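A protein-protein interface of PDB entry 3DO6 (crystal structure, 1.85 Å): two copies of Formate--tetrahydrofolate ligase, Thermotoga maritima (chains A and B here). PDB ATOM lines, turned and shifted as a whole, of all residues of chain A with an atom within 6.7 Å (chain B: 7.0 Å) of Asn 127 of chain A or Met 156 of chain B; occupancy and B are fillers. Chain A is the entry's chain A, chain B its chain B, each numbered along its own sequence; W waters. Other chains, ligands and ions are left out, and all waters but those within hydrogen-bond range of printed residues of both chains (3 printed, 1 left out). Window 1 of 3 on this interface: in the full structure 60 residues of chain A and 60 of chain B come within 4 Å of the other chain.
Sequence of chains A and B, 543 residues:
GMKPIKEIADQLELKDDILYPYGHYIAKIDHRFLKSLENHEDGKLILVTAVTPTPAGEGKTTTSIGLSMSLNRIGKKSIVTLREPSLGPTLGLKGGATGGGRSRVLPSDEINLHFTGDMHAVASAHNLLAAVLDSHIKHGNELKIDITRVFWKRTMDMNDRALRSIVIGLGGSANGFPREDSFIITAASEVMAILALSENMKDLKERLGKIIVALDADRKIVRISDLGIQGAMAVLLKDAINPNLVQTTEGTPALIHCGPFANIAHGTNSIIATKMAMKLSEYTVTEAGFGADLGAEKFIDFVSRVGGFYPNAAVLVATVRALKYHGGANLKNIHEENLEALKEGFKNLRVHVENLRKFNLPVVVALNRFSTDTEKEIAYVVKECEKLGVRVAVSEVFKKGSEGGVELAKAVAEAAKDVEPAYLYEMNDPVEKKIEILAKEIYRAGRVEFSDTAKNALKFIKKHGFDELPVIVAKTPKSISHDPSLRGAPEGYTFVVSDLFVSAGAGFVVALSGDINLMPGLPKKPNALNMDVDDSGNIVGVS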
ATOM      1  N   VAL A 122     -21.565  25.370   5.320  1.00  0.00           N
ATOM      2  CA  VAL A 122     -20.635  24.252   5.295  1.00  0.00           C
ATOM      3  C   VAL A 122     -19.416  24.589   6.150  1.00  0.00           C
ATOM      4  O   VAL A 122     -18.979  23.762   6.981  1.00  0.00           O
ATOM      5  CB  VAL A 122     -20.234  23.833   3.841  1.00  0.00           C
ATOM      6  CG1 VAL A 122     -19.101  22.814   3.837  1.00  0.00           C
ATOM      7  CG2 VAL A 122     -21.481  23.266   3.099  1.00  0.00           C
ATOM      8  N   ALA A 123     -18.890  25.799   5.973  1.00  0.00           N
ATOM      9  CA  ALA A 123     -17.690  26.205   6.716  1.00  0.00           C
ATOM     10  C   ALA A 123     -17.955  26.179   8.219  1.00  0.00           C
ATOM     11  O   ALA A 123     -17.150  25.705   8.978  1.00  0.00           O
ATOM     12  CB  ALA A 123     -17.165  27.574   6.253  1.00  0.00           C
ATOM     13  N   SER A 124     -19.120  26.672   8.613  1.00  0.00           N
ATOM     14  CA  SER A 124     -19.529  26.717  10.014  1.00  0.00           C
ATOM     15  C   SER A 124     -19.580  25.345  10.655  1.00  0.00           C
ATOM     16  O   SER A 124     -19.078  25.128  11.751  1.00  0.00           O
ATOM     17  CB  SER A 124     -20.915  27.357  10.130  1.00  0.00           C
ATOM     18  OG  SER A 124     -20.838  28.765  10.021  1.00  0.00           O
ATOM     19  N   ALA A 125     -20.257  24.441   9.973  1.00  0.00           N
ATOM     20  CA  ALA A 125     -20.372  23.055  10.431  1.00  0.00           C
ATOM     21  C   ALA A 125     -18.994  22.385  10.533  1.00  0.00           C
ATOM     22  O   ALA A 125     -18.662  21.733  11.523  1.00  0.00           O
ATOM     23  CB  ALA A 125     -21.304  22.219   9.515  1.00  0.00           C
ATOM     24  N   HIS A 126     -18.182  22.601   9.508  1.00  0.00           N
ATOM     25  CA  HIS A 126     -16.852  21.981   9.413  1.00  0.00           C
ATOM     26  C   HIS A 126     -15.948  22.457  10.548  1.00  0.00           C
ATOM     27  O   HIS A 126     -15.291  21.677  11.256  1.00  0.00           O
ATOM     28  CB  HIS A 126     -16.201  22.381   8.082  1.00  0.00           C
ATOM     29  CG  HIS A 126     -14.940  21.633   7.763  1.00  0.00           C
ATOM     30  ND1 HIS A 126     -14.860  20.718   6.735  1.00  0.00           N
ATOM     31  CD2 HIS A 126     -13.706  21.673   8.333  1.00  0.00           C
ATOM     32  CE1 HIS A 126     -13.637  20.220   6.690  1.00  0.00           C
ATOM     33  NE2 HIS A 126     -12.914  20.786   7.650  1.00  0.00           N
ATOM     34  N   ASN A 127     -15.947  23.771  10.713  1.00  0.00           N
ATOM     35  CA  ASN A 127     -15.113  24.444  11.740  1.00  0.00           C
ATOM     36  C   ASN A 127     -15.560  24.190  13.165  1.00  0.00           C
ATOM     37  O   ASN A 127     -14.763  24.196  14.077  1.00  0.00           O
ATOM     38  CB  ASN A 127     -14.956  25.934  11.435  1.00  0.00           C
ATOM     39  CG  ASN A 127     -14.006  26.172  10.238  1.00  0.00           C
ATOM     40  OD1 ASN A 127     -13.153  25.330   9.920  1.00  0.00           O
ATOM     41  ND2 ASN A 127     -14.186  27.281   9.563  1.00  0.00           N
ATOM     42  N   LEU A 128     -16.869  23.979  13.331  1.00  0.00           N
ATOM     43  CA  LEU A 128     -17.432  23.596  14.622  1.00  0.00           C
ATOM     44  C   LEU A 128     -16.800  22.277  15.093  1.00  0.00           C
ATOM     45  O   LEU A 128     -16.385  22.162  16.249  1.00  0.00           O
ATOM     46  CB  LEU A 128     -18.975  23.507  14.578  1.00  0.00           C
ATOM     47  CG  LEU A 128     -19.635  22.781  15.776  1.00  0.00           C
ATOM     48  CD1 LEU A 128     -19.339  23.574  17.033  1.00  0.00           C
ATOM     49  CD2 LEU A 128     -21.135  22.540  15.598  1.00  0.00           C
ATOM     50  N   LEU A 129     -16.679  21.318  14.184  1.00  0.00           N
ATOM     51  CA  LEU A 129     -16.132  20.027  14.548  1.00  0.00           C
ATOM     52  C   LEU A 129     -14.695  20.237  15.006  1.00  0.00           C
ATOM     53  O   LEU A 129     -14.298  19.782  16.071  1.00  0.00           O
ATOM     54  CB  LEU A 129     -16.178  19.041  13.386  1.00  0.00           C
ATOM     55  CG  LEU A 129     -15.354  17.757  13.527  1.00  0.00           C
ATOM     56  CD1 LEU A 129     -15.802  16.902  14.725  1.00  0.00           C
ATOM     57  CD2 LEU A 129     -15.468  16.969  12.224  1.00  0.00           C
ATOM     58  N   ALA A 130     -13.942  20.973  14.204  1.00  0.00           N
ATOM     59  CA  ALA A 130     -12.524  21.246  14.538  1.00  0.00           C
ATOM     60  C   ALA A 130     -12.412  21.863  15.961  1.00  0.00           C
ATOM     61  O   ALA A 130     -11.602  21.429  16.824  1.00  0.00           O
ATOM     62  CB  ALA A 130     -11.883  22.167  13.466  1.00  0.00           C
ATOM     63  N   ALA A 131     -13.255  22.860  16.216  1.00  0.00           N
ATOM     64  CA  ALA A 131     -13.262  23.564  17.498  1.00  0.00           C
ATOM     65  C   ALA A 131     -13.576  22.612  18.642  1.00  0.00           C
ATOM     66  O   ALA A 131     -12.926  22.625  19.700  1.00  0.00           O
ATOM     67  CB  ALA A 131     -14.276  24.770  17.487  1.00  0.00           C
ATOM     68  N   VAL A 132     -14.572  21.778  18.403  1.00  0.00           N
ATOM     69  CA  VAL A 132     -15.031  20.820  19.392  1.00  0.00           C
ATOM     70  C   VAL A 132     -13.952  19.743  19.638  1.00  0.00           C
ATOM     71  O   VAL A 132     -13.757  19.259  20.763  1.00  0.00           O
ATOM     72  CB  VAL A 132     -16.418  20.161  19.000  1.00  0.00           C
ATOM     73  CG1 VAL A 132     -16.659  18.850  19.776  1.00  0.00           C
ATOM     74  CG2 VAL A 132     -17.621  21.207  19.154  1.00  0.00           C
ATOM     75  N   TRP A 152      -8.757  15.577  10.250  1.00  0.00           N
ATOM     76  CA  TRP A 152      -9.705  16.715  10.085  1.00  0.00           C
ATOM     77  C   TRP A 152      -8.966  18.024  10.109  1.00  0.00           C
ATOM     78  O   TRP A 152      -8.150  18.263  10.994  1.00  0.00           O
ATOM     79  CB  TRP A 152     -10.773  16.737  11.182  1.00  0.00           C
ATOM     80  CG  TRP A 152     -11.956  17.583  10.850  1.00  0.00           C
ATOM     81  CD1 TRP A 152     -12.276  18.788  11.392  1.00  0.00           C
ATOM     82  CD2 TRP A 152     -12.966  17.298   9.883  1.00  0.00           C
ATOM     83  NE1 TRP A 152     -13.443  19.250  10.851  1.00  0.00           N
ATOM     84  CE2 TRP A 152     -13.883  18.366   9.909  1.00  0.00           C
ATOM     85  CE3 TRP A 152     -13.203  16.227   9.006  1.00  0.00           C
ATOM     86  CZ2 TRP A 152     -15.012  18.397   9.088  1.00  0.00           C
ATOM     87  CZ3 TRP A 152     -14.301  16.289   8.163  1.00  0.00           C
ATOM     88  CH2 TRP A 152     -15.184  17.371   8.208  1.00  0.00           C
ATOM     89  N   LYS A 153      -9.244  18.834   9.083  1.00  0.00           N
ATOM     90  CA  LYS A 153      -8.623  20.143   8.894  1.00  0.00           C
ATOM     91  C   LYS A 153      -9.661  21.255   9.168  1.00  0.00           C
ATOM     92  O   LYS A 153     -10.836  21.013   9.390  1.00  0.00           O
ATOM     93  CB  LYS A 153      -8.029  20.298   7.487  1.00  0.00           C
ATOM     94  CG  LYS A 153      -7.123  19.162   7.007  1.00  0.00           C
ATOM     95  CD  LYS A 153      -6.219  18.696   8.122  1.00  0.00           C
ATOM     96  CE  LYS A 153      -5.188  17.627   7.668  1.00  0.00           C
ATOM     97  NZ  LYS A 153      -4.409  16.929   8.800  1.00  0.00           N
ATOM     98  N   ARG A 154      -9.199  22.489   9.168  1.00  0.00           N
ATOM     99  CA  ARG A 154     -10.116  23.580   9.225  1.00  0.00           C
ATOM    100  C   ARG A 154     -10.399  24.057   7.800  1.00  0.00           C
ATOM    101  O   ARG A 154      -9.765  23.592   6.849  1.00  0.00           O
ATOM    102  CB  ARG A 154      -9.634  24.681  10.119  1.00  0.00           C
ATOM    103  CG  ARG A 154      -9.887  24.388  11.613  1.00  0.00           C
ATOM    104  CD  ARG A 154      -9.092  25.298  12.558  1.00  0.00           C
ATOM    105  NE  ARG A 154      -9.600  25.153  13.929  1.00  0.00           N
ATOM    106  CZ  ARG A 154      -9.185  24.221  14.788  1.00  0.00           C
ATOM    107  NH1 ARG A 154      -8.238  23.380  14.459  1.00  0.00           N
ATOM    108  NH2 ARG A 154      -9.712  24.132  15.982  1.00  0.00           N
ATOM    109  N   THR A 155     -11.320  25.020   7.717  1.00  0.00           N
ATOM    110  CA  THR A 155     -11.789  25.522   6.451  1.00  0.00           C
ATOM    111  C   THR A 155     -12.090  27.007   6.392  1.00  0.00           C
ATOM    112  O   THR A 155     -12.473  27.667   7.376  1.00  0.00           O
ATOM    113  CB  THR A 155     -12.972  24.692   5.949  1.00  0.00           C
ATOM    114  OG1 THR A 155     -13.064  24.881   4.534  1.00  0.00           O
ATOM    115  CG2 THR A 155     -14.285  25.037   6.689  1.00  0.00           C
ATOM    116  N   MET A 156     -11.846  27.534   5.205  1.00  0.00           N
ATOM    117  CA  MET A 156     -12.377  28.861   4.814  1.00  0.00           C
ATOM    118  C   MET A 156     -12.555  29.007   3.296  1.00  0.00           C
ATOM    119  O   MET A 156     -11.884  28.357   2.515  1.00  0.00           O
ATOM    120  CB  MET A 156     -11.576  30.035   5.428  1.00  0.00           C
ATOM    121  CG  MET A 156     -10.278  30.438   4.870  1.00  0.00           C
ATOM    122  SD  MET A 156      -9.839  32.297   5.401  1.00  0.00           S
ATOM    123  CE  MET A 156      -9.746  32.172   7.365  1.00  0.00           C
ATOM    124  N   PHE A 183      -5.678  24.549   6.780  1.00  0.00           N
ATOM    125  CA  PHE A 183      -6.954  24.969   6.226  1.00  0.00           C
ATOM    126  C   PHE A 183      -7.021  24.510   4.768  1.00  0.00           C
ATOM    127  O   PHE A 183      -6.059  24.649   3.996  1.00  0.00           O
ATOM    128  CB  PHE A 183      -7.158  26.500   6.270  1.00  0.00           C
ATOM    129  CG  PHE A 183      -7.587  27.077   7.612  1.00  0.00           C
ATOM    130  CD1 PHE A 183      -6.738  27.069   8.701  1.00  0.00           C
ATOM    131  CD2 PHE A 183      -8.835  27.689   7.758  1.00  0.00           C
ATOM    132  CE1 PHE A 183      -7.125  27.625   9.900  1.00  0.00           C
ATOM    133  CE2 PHE A 183      -9.225  28.271   8.980  1.00  0.00           C
ATOM    134  CZ  PHE A 183      -8.367  28.251  10.042  1.00  0.00           C
ATOM    135  N   THR A 186     -13.279  25.670   1.377  1.00  0.00           N
ATOM    136  CA  THR A 186     -14.485  25.054   1.907  1.00  0.00           C
ATOM    137  C   THR A 186     -15.113  24.042   0.952  1.00  0.00           C
ATOM    138  O   THR A 186     -15.657  23.038   1.372  1.00  0.00           O
ATOM    139  CB  THR A 186     -15.482  26.122   2.299  1.00  0.00           C
ATOM    140  OG1 THR A 186     -14.867  26.971   3.286  1.00  0.00           O
ATOM    141  CG2 THR A 186     -16.763  25.515   2.842  1.00  0.00           C
ATOM    142  N   MET A 233     -24.157  19.945  13.504  1.00  0.00           N
ATOM    143  CA  MET A 233     -23.699  20.243  12.132  1.00  0.00           C
ATOM    144  C   MET A 233     -24.894  20.223  11.156  1.00  0.00           C
ATOM    145  O   MET A 233     -25.045  21.077  10.276  1.00  0.00           O
ATOM    146  CB  MET A 233     -22.633  19.225  11.708  1.00  0.00           C
ATOM    147  CG  MET A 233     -21.322  19.284  12.529  1.00  0.00           C
ATOM    148  SD  MET A 233     -20.108  17.832  12.206  1.00  0.00           S
ATOM    149  CE  MET A 233     -19.335  18.443  10.514  1.00  0.00           C
ATOM    150  N   GLY B  88     -21.112  31.751  17.409  1.00  0.00           N
ATOM    151  CA  GLY B  88     -20.150  31.050  18.245  1.00  0.00           C
ATOM    152  C   GLY B  88     -20.624  30.701  19.657  1.00  0.00           C
ATOM    153  O   GLY B  88     -20.627  29.547  20.055  1.00  0.00           O
ATOM    154  N   ALA B 123     -16.939  38.484   8.213  1.00  0.00           N
ATOM    155  CA  ALA B 123     -15.785  37.538   8.290  1.00  0.00           C
ATOM    156  C   ALA B 123     -15.034  37.437   6.965  1.00  0.00           C
ATOM    157  O   ALA B 123     -13.807  37.518   6.904  1.00  0.00           O
ATOM    158  CB  ALA B 123     -16.261  36.105   8.791  1.00  0.00           C
ATOM    159  N   HIS B 126     -13.063  40.568   6.277  1.00  0.00           N
ATOM    160  CA  HIS B 126     -11.996  40.659   7.297  1.00  0.00           C
ATOM    161  C   HIS B 126     -10.839  39.760   6.900  1.00  0.00           C
ATOM    162  O   HIS B 126      -9.649  40.162   6.894  1.00  0.00           O
ATOM    163  CB  HIS B 126     -12.520  40.283   8.691  1.00  0.00           C
ATOM    164  CG  HIS B 126     -11.520  40.491   9.802  1.00  0.00           C
ATOM    165  ND1 HIS B 126     -11.729  41.373  10.846  1.00  0.00           N
ATOM    166  CD2 HIS B 126     -10.310  39.923  10.032  1.00  0.00           C
ATOM    167  CE1 HIS B 126     -10.690  41.345  11.664  1.00  0.00           C
ATOM    168  NE2 HIS B 126      -9.811  40.476  11.190  1.00  0.00           N
ATOM    169  N   ASN B 127     -11.210  38.527   6.597  1.00  0.00           N
ATOM    170  CA  ASN B 127     -10.253  37.502   6.188  1.00  0.00           C
ATOM    171  C   ASN B 127      -9.636  37.750   4.821  1.00  0.00           C
ATOM    172  O   ASN B 127      -8.522  37.290   4.556  1.00  0.00           O
ATOM    173  CB  ASN B 127     -10.862  36.097   6.290  1.00  0.00           C
ATOM    174  CG  ASN B 127     -10.990  35.657   7.743  1.00  0.00           C
ATOM    175  OD1 ASN B 127     -10.258  36.179   8.605  1.00  0.00           O
ATOM    176  ND2 ASN B 127     -11.931  34.763   8.040  1.00  0.00           N
ATOM    177  N   ARG B 154      -6.948  37.399  11.993  1.00  0.00           N
ATOM    178  CA  ARG B 154      -7.976  36.677  11.281  1.00  0.00           C
ATOM    179  C   ARG B 154      -9.212  36.514  12.173  1.00  0.00           C
ATOM    180  O   ARG B 154      -9.226  36.855  13.362  1.00  0.00           O
ATOM    181  CB  ARG B 154      -7.463  35.330  10.719  1.00  0.00           C
ATOM    182  CG  ARG B 154      -6.579  35.564   9.478  1.00  0.00           C
ATOM    183  CD  ARG B 154      -5.823  34.319   8.993  1.00  0.00           C
ATOM    184  NE  ARG B 154      -5.306  34.481   7.626  1.00  0.00           N
ATOM    185  CZ  ARG B 154      -4.138  35.037   7.354  1.00  0.00           C
ATOM    186  NH1 ARG B 154      -3.395  35.527   8.330  1.00  0.00           N
ATOM    187  NH2 ARG B 154      -3.748  35.165   6.110  1.00  0.00           N
ATOM    188  N   THR B 155     -10.282  36.034  11.554  1.00  0.00           N
ATOM    189  CA  THR B 155     -11.551  35.968  12.239  1.00  0.00           C
ATOM    190  C   THR B 155     -12.380  34.725  11.877  1.00  0.00           C
ATOM    191  O   THR B 155     -12.351  34.188  10.751  1.00  0.00           O
ATOM    192  CB  THR B 155     -12.365  37.289  12.047  1.00  0.00           C
ATOM    193  OG1 THR B 155     -13.310  37.395  13.114  1.00  0.00           O
ATOM    194  CG2 THR B 155     -13.031  37.301  10.681  1.00  0.00           C
ATOM    195  N   MET B 156     -13.102  34.256  12.881  1.00  0.00           N
ATOM    196  CA  MET B 156     -14.216  33.296  12.673  1.00  0.00           C
ATOM    197  C   MET B 156     -15.276  33.455  13.736  1.00  0.00           C
ATOM    198  O   MET B 156     -15.011  33.955  14.834  1.00  0.00           O
ATOM    199  CB  MET B 156     -13.760  31.836  12.534  1.00  0.00           C
ATOM    200  CG  MET B 156     -13.232  31.098  13.670  1.00  0.00           C
ATOM    201  SD  MET B 156     -13.323  29.143  13.300  1.00  0.00           S
ATOM    202  CE  MET B 156     -11.975  28.939  11.886  1.00  0.00           C
ATOM    203  N   ASP B 157     -16.500  33.116  13.371  1.00  0.00           N
ATOM    204  CA  ASP B 157     -17.593  33.217  14.330  1.00  0.00           C
ATOM    205  C   ASP B 157     -17.836  31.849  14.963  1.00  0.00           C
ATOM    206  O   ASP B 157     -18.769  31.092  14.649  1.00  0.00           O
ATOM    207  CB  ASP B 157     -18.864  33.788  13.700  1.00  0.00           C
ATOM    208  CG  ASP B 157     -19.918  34.058  14.732  1.00  0.00           C
ATOM    209  OD1 ASP B 157     -19.573  34.002  15.942  1.00  0.00           O
ATOM    210  OD2 ASP B 157     -21.072  34.323  14.331  1.00  0.00           O
ATOM    211  N   MET B 158     -16.920  31.575  15.863  1.00  0.00           N
ATOM    212  CA  MET B 158     -16.784  30.301  16.497  1.00  0.00           C
ATOM    213  C   MET B 158     -15.977  30.542  17.733  1.00  0.00           C
ATOM    214  O   MET B 158     -15.045  31.327  17.730  1.00  0.00           O
ATOM    215  CB  MET B 158     -16.001  29.349  15.577  1.00  0.00           C
ATOM    216  CG  MET B 158     -15.967  27.884  16.003  1.00  0.00           C
ATOM    217  SD  MET B 158     -17.733  27.033  15.925  1.00  0.00           S
ATOM    218  CE  MET B 158     -18.131  27.313  14.071  1.00  0.00           C
ATOM    219  N   ASN B 159     -16.348  29.839  18.780  1.00  0.00           N
ATOM    220  CA  ASN B 159     -15.647  29.890  20.085  1.00  0.00           C
ATOM    221  C   ASN B 159     -14.501  28.879  20.053  1.00  0.00           C
ATOM    222  O   ASN B 159     -14.672  27.740  20.491  1.00  0.00           O
ATOM    223  CB  ASN B 159     -16.596  29.508  21.253  1.00  0.00           C
ATOM    224  CG  ASN B 159     -17.500  30.634  21.686  1.00  0.00           C
ATOM    225  OD1 ASN B 159     -17.878  31.481  20.891  1.00  0.00           O
ATOM    226  ND2 ASN B 159     -17.872  30.633  22.973  1.00  0.00           N
ATOM    227  N   ASP B 160     -13.367  29.299  19.491  1.00  0.00           N
ATOM    228  CA  ASP B 160     -12.219  28.407  19.277  1.00  0.00           C
ATOM    229  C   ASP B 160     -10.911  28.896  19.917  1.00  0.00           C
ATOM    230  O   ASP B 160     -10.067  29.603  19.320  1.00  0.00           O
ATOM    231  CB  ASP B 160     -12.051  28.118  17.784  1.00  0.00           C
ATOM    232  CG  ASP B 160     -11.260  26.859  17.537  1.00  0.00           C
ATOM    233  OD1 ASP B 160     -10.644  26.341  18.503  1.00  0.00           O
ATOM    234  OD2 ASP B 160     -11.241  26.364  16.389  1.00  0.00           O
ATOM    235  N   LEU B 163      -7.297  28.842  18.343  1.00  0.00           N
ATOM    236  CA  LEU B 163      -6.865  29.820  17.335  1.00  0.00           C
ATOM    237  C   LEU B 163      -6.408  31.167  17.925  1.00  0.00           C
ATOM    238  O   LEU B 163      -6.098  32.098  17.211  1.00  0.00           O
ATOM    239  CB  LEU B 163      -7.972  30.037  16.291  1.00  0.00           C
ATOM    240  CG  LEU B 163      -8.417  28.760  15.562  1.00  0.00           C
ATOM    241  CD1 LEU B 163      -9.502  29.033  14.543  1.00  0.00           C
ATOM    242  CD2 LEU B 163      -7.256  28.069  14.865  1.00  0.00           C
ATOM    243  N   PHE B 183      -6.702  34.478  15.660  1.00  0.00           N
ATOM    244  CA  PHE B 183      -8.114  34.666  15.310  1.00  0.00           C
ATOM    245  C   PHE B 183      -8.864  35.295  16.496  1.00  0.00           C
ATOM    246  O   PHE B 183      -8.636  34.984  17.675  1.00  0.00           O
ATOM    247  CB  PHE B 183      -8.817  33.351  14.956  1.00  0.00           C
ATOM    248  CG  PHE B 183      -8.516  32.814  13.589  1.00  0.00           C
ATOM    249  CD1 PHE B 183      -7.237  32.330  13.257  1.00  0.00           C
ATOM    250  CD2 PHE B 183      -9.530  32.718  12.647  1.00  0.00           C
ATOM    251  CE1 PHE B 183      -7.000  31.791  12.018  1.00  0.00           C
ATOM    252  CE2 PHE B 183      -9.331  32.175  11.420  1.00  0.00           C
ATOM    253  CZ  PHE B 183      -8.040  31.711  11.075  1.00  0.00           C
ATOM    254  N   ILE B 184      -9.749  36.201  16.126  1.00  0.00           N
ATOM    255  CA  ILE B 184     -10.690  36.851  17.027  1.00  0.00           C
ATOM    256  C   ILE B 184     -12.102  36.477  16.568  1.00  0.00           C
ATOM    257  O   ILE B 184     -12.329  36.239  15.387  1.00  0.00           O
ATOM    258  CB  ILE B 184     -10.486  38.394  17.104  1.00  0.00           C
ATOM    259  CG1 ILE B 184     -10.767  39.086  15.760  1.00  0.00           C
ATOM    260  CG2 ILE B 184      -9.119  38.728  17.743  1.00  0.00           C
ATOM    261  CD1 ILE B 184     -10.824  40.616  15.807  1.00  0.00           C
ATOM    262  N   ILE B 185     -13.042  36.384  17.504  1.00  0.00           N
ATOM    263  CA  ILE B 185     -14.436  36.130  17.121  1.00  0.00           C
ATOM    264  C   ILE B 185     -14.967  37.323  16.283  1.00  0.00           C
ATOM    265  O   ILE B 185     -14.568  38.465  16.472  1.00  0.00           O
ATOM    266  CB  ILE B 185     -15.319  35.818  18.339  1.00  0.00           C
ATOM    267  CG1 ILE B 185     -16.512  34.973  17.890  1.00  0.00           C
ATOM    268  CG2 ILE B 185     -15.666  37.079  19.068  1.00  0.00           C
ATOM    269  CD1 ILE B 185     -17.003  34.025  18.954  1.00  0.00           C
ATOM    270  N   THR B 186     -15.772  37.014  15.285  1.00  0.00           N
ATOM    271  CA  THR B 186     -16.095  37.978  14.230  1.00  0.00           C
ATOM    272  C   THR B 186     -16.707  39.262  14.794  1.00  0.00           C
ATOM    273  O   THR B 186     -16.405  40.371  14.341  1.00  0.00           O
ATOM    274  CB  THR B 186     -16.965  37.318  13.115  1.00  0.00           C
ATOM    275  OG1 THR B 186     -16.281  36.152  12.621  1.00  0.00           O
ATOM    276  CG2 THR B 186     -17.197  38.284  11.939  1.00  0.00           C
ATOM    277  N   ALA B 187     -17.501  39.104  15.838  1.00  0.00           N
ATOM    278  CA  ALA B 187     -18.132  40.253  16.489  1.00  0.00           C
ATOM    279  C   ALA B 187     -17.107  41.331  16.852  1.00  0.00           C
ATOM    280  O   ALA B 187     -17.442  42.538  16.831  1.00  0.00           O
ATOM    281  CB  ALA B 187     -18.904  39.837  17.714  1.00  0.00           C
ATOM    282  N   LEU B 518     -11.021  38.113  23.373  1.00  0.00           N
ATOM    283  CA  LEU B 518     -11.650  38.330  22.060  1.00  0.00           C
ATOM    284  C   LEU B 518     -11.863  37.034  21.287  1.00  0.00           C
ATOM    285  O   LEU B 518     -12.298  37.047  20.137  1.00  0.00           O
ATOM    286  CB  LEU B 518     -10.849  39.288  21.203  1.00  0.00           C
ATOM    287  CG  LEU B 518     -10.630  40.670  21.811  1.00  0.00           C
ATOM    288  CD1 LEU B 518      -9.943  41.533  20.773  1.00  0.00           C
ATOM    289  CD2 LEU B 518     -11.933  41.300  22.253  1.00  0.00           C
ATOM    290  N   MET B 519     -11.577  35.920  21.952  1.00  0.00           N
ATOM    291  CA  MET B 519     -11.894  34.598  21.407  1.00  0.00           C
ATOM    292  C   MET B 519     -12.298  33.648  22.523  1.00  0.00           C
ATOM    293  O   MET B 519     -11.472  32.930  23.061  1.00  0.00           O
ATOM    294  CB  MET B 519     -10.697  34.049  20.604  1.00  0.00           C
ATOM    295  CG  MET B 519     -10.945  32.693  19.954  1.00  0.00           C
ATOM    296  SD  MET B 519     -12.610  32.601  18.940  1.00  0.00           S
ATOM    297  CE  MET B 519     -11.800  32.869  17.170  1.00  0.00           C
HETATM  298  O   HOH W   1      -7.596  34.808   5.715  1.00  0.00           O
HETATM  299  O   HOH W   2     -19.889  30.657  11.948  1.00  0.00           O
HETATM  300  O   HOH W   3     -11.450  24.721  20.475  1.00  0.00           O
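NH2 of Arg 154 of chain A lies within salt-bridge range of OD2 of Asp 160 of chain B, 2.7 Å away.
The side-chain amide nitrogen (ND2) of Asn 127 of chain A sits at hydrogen-bond distance from the backbone carbonyl oxygen (O) of Thr 155 of chain A (2.8 Å).
The backbone carbonyl oxygen (O) of Met 156 of chain B is in hydrogen-bond range of the backbone NH (N) of Thr 186 of chain B (3.2 Å).
O of Leu 163 of chain B is in hydrogen-bond range of N of Phe 183 of chain B (2.9 Å).
Among the printed residues, pairs that only touch across the chains: Ser 124 of chain A with Met 158 of chain B, Asn 127 of chain A with Met 156 of chain B, Leu 128 of chain A with Met 158 of chain B, Ala 131 of chain A with Met 158 of chain B, Ala 131 of chain A with Asp 160 of chain B, Arg 154 of chain A with Leu 163 of chain B, Met 156 of chain A with Asn 127 of chain B and Phe 183 of chain A with Phe 183 of chain B.
Met 156 of chain B touches just one residue of chain A: Asn 127 (3.6 Å).
Of the printed residues of chain A, Phe 183 of chain B touches Phe 183.
Of the printed residues of chain B, Leu 128 of chain A touches Met 158.
Of the printed residues of chain B, Phe 183 of chain A touches Phe 183.
The nearest residue of chain B that does not touch Asn 127 of chain A is Met 158 of chain B (4.1 Å).
The nearest printed residue of chain B that does not touch Ser 124 of chain A is Asp 157 of chain B (5.6 Å).
Of the 19 printed residues of chain A, 7 touch a printed residue of chain B.
Printed residues of chain A that touch a printed residue of chain B: Ser 124, Asn 127, Leu 128, Ala 131, Arg 154, Met 156 and Phe 183.
Printed residues of chain B that touch a printed residue of chain A: Asn 127, Met 156, Met 158, Asp 160, Leu 163 and Phe 183.
Hydrophobic or aromatic side chains of chain B within 4 Å of the printed part of chain A: Met 156, Met 158, Leu 163 and Phe 183.
Among the printed residues, Asp or Glu carboxylates within 4 Å of a Lys or Arg side-chain nitrogen of the other chain: Arg 154 of chain A with Asp 160 of chain B (2.7 Å).
Asn 127 of chain A touches Met 156 of chain B, and with the chains exchanged Met 156 of chain A touches Asn 127 of chain B.
Phe 183 of chain A touches its own counterpart, Phe 183 of chain B.
Positions printed for both chains: 123, 126, 127, 154, 155, 156, 183 and 186.
Water W3 bridges OD1 of Asp 160 of chain B and O of Ala 131 of chain A.
Water W2 bridges the side-chain hydroxyl of Ser 124 of chain A (2.9 Å) and the backbone carbonyl oxygen of Asp 157 of chain B (3.0 Å).
Water W1 lies within hydrogen-bond range of O of Asn 127 of chain B (2.9 Å), NE of Arg 154 of chain B (3.0 Å) and SD of Met 156 of chain A (3.4 Å).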
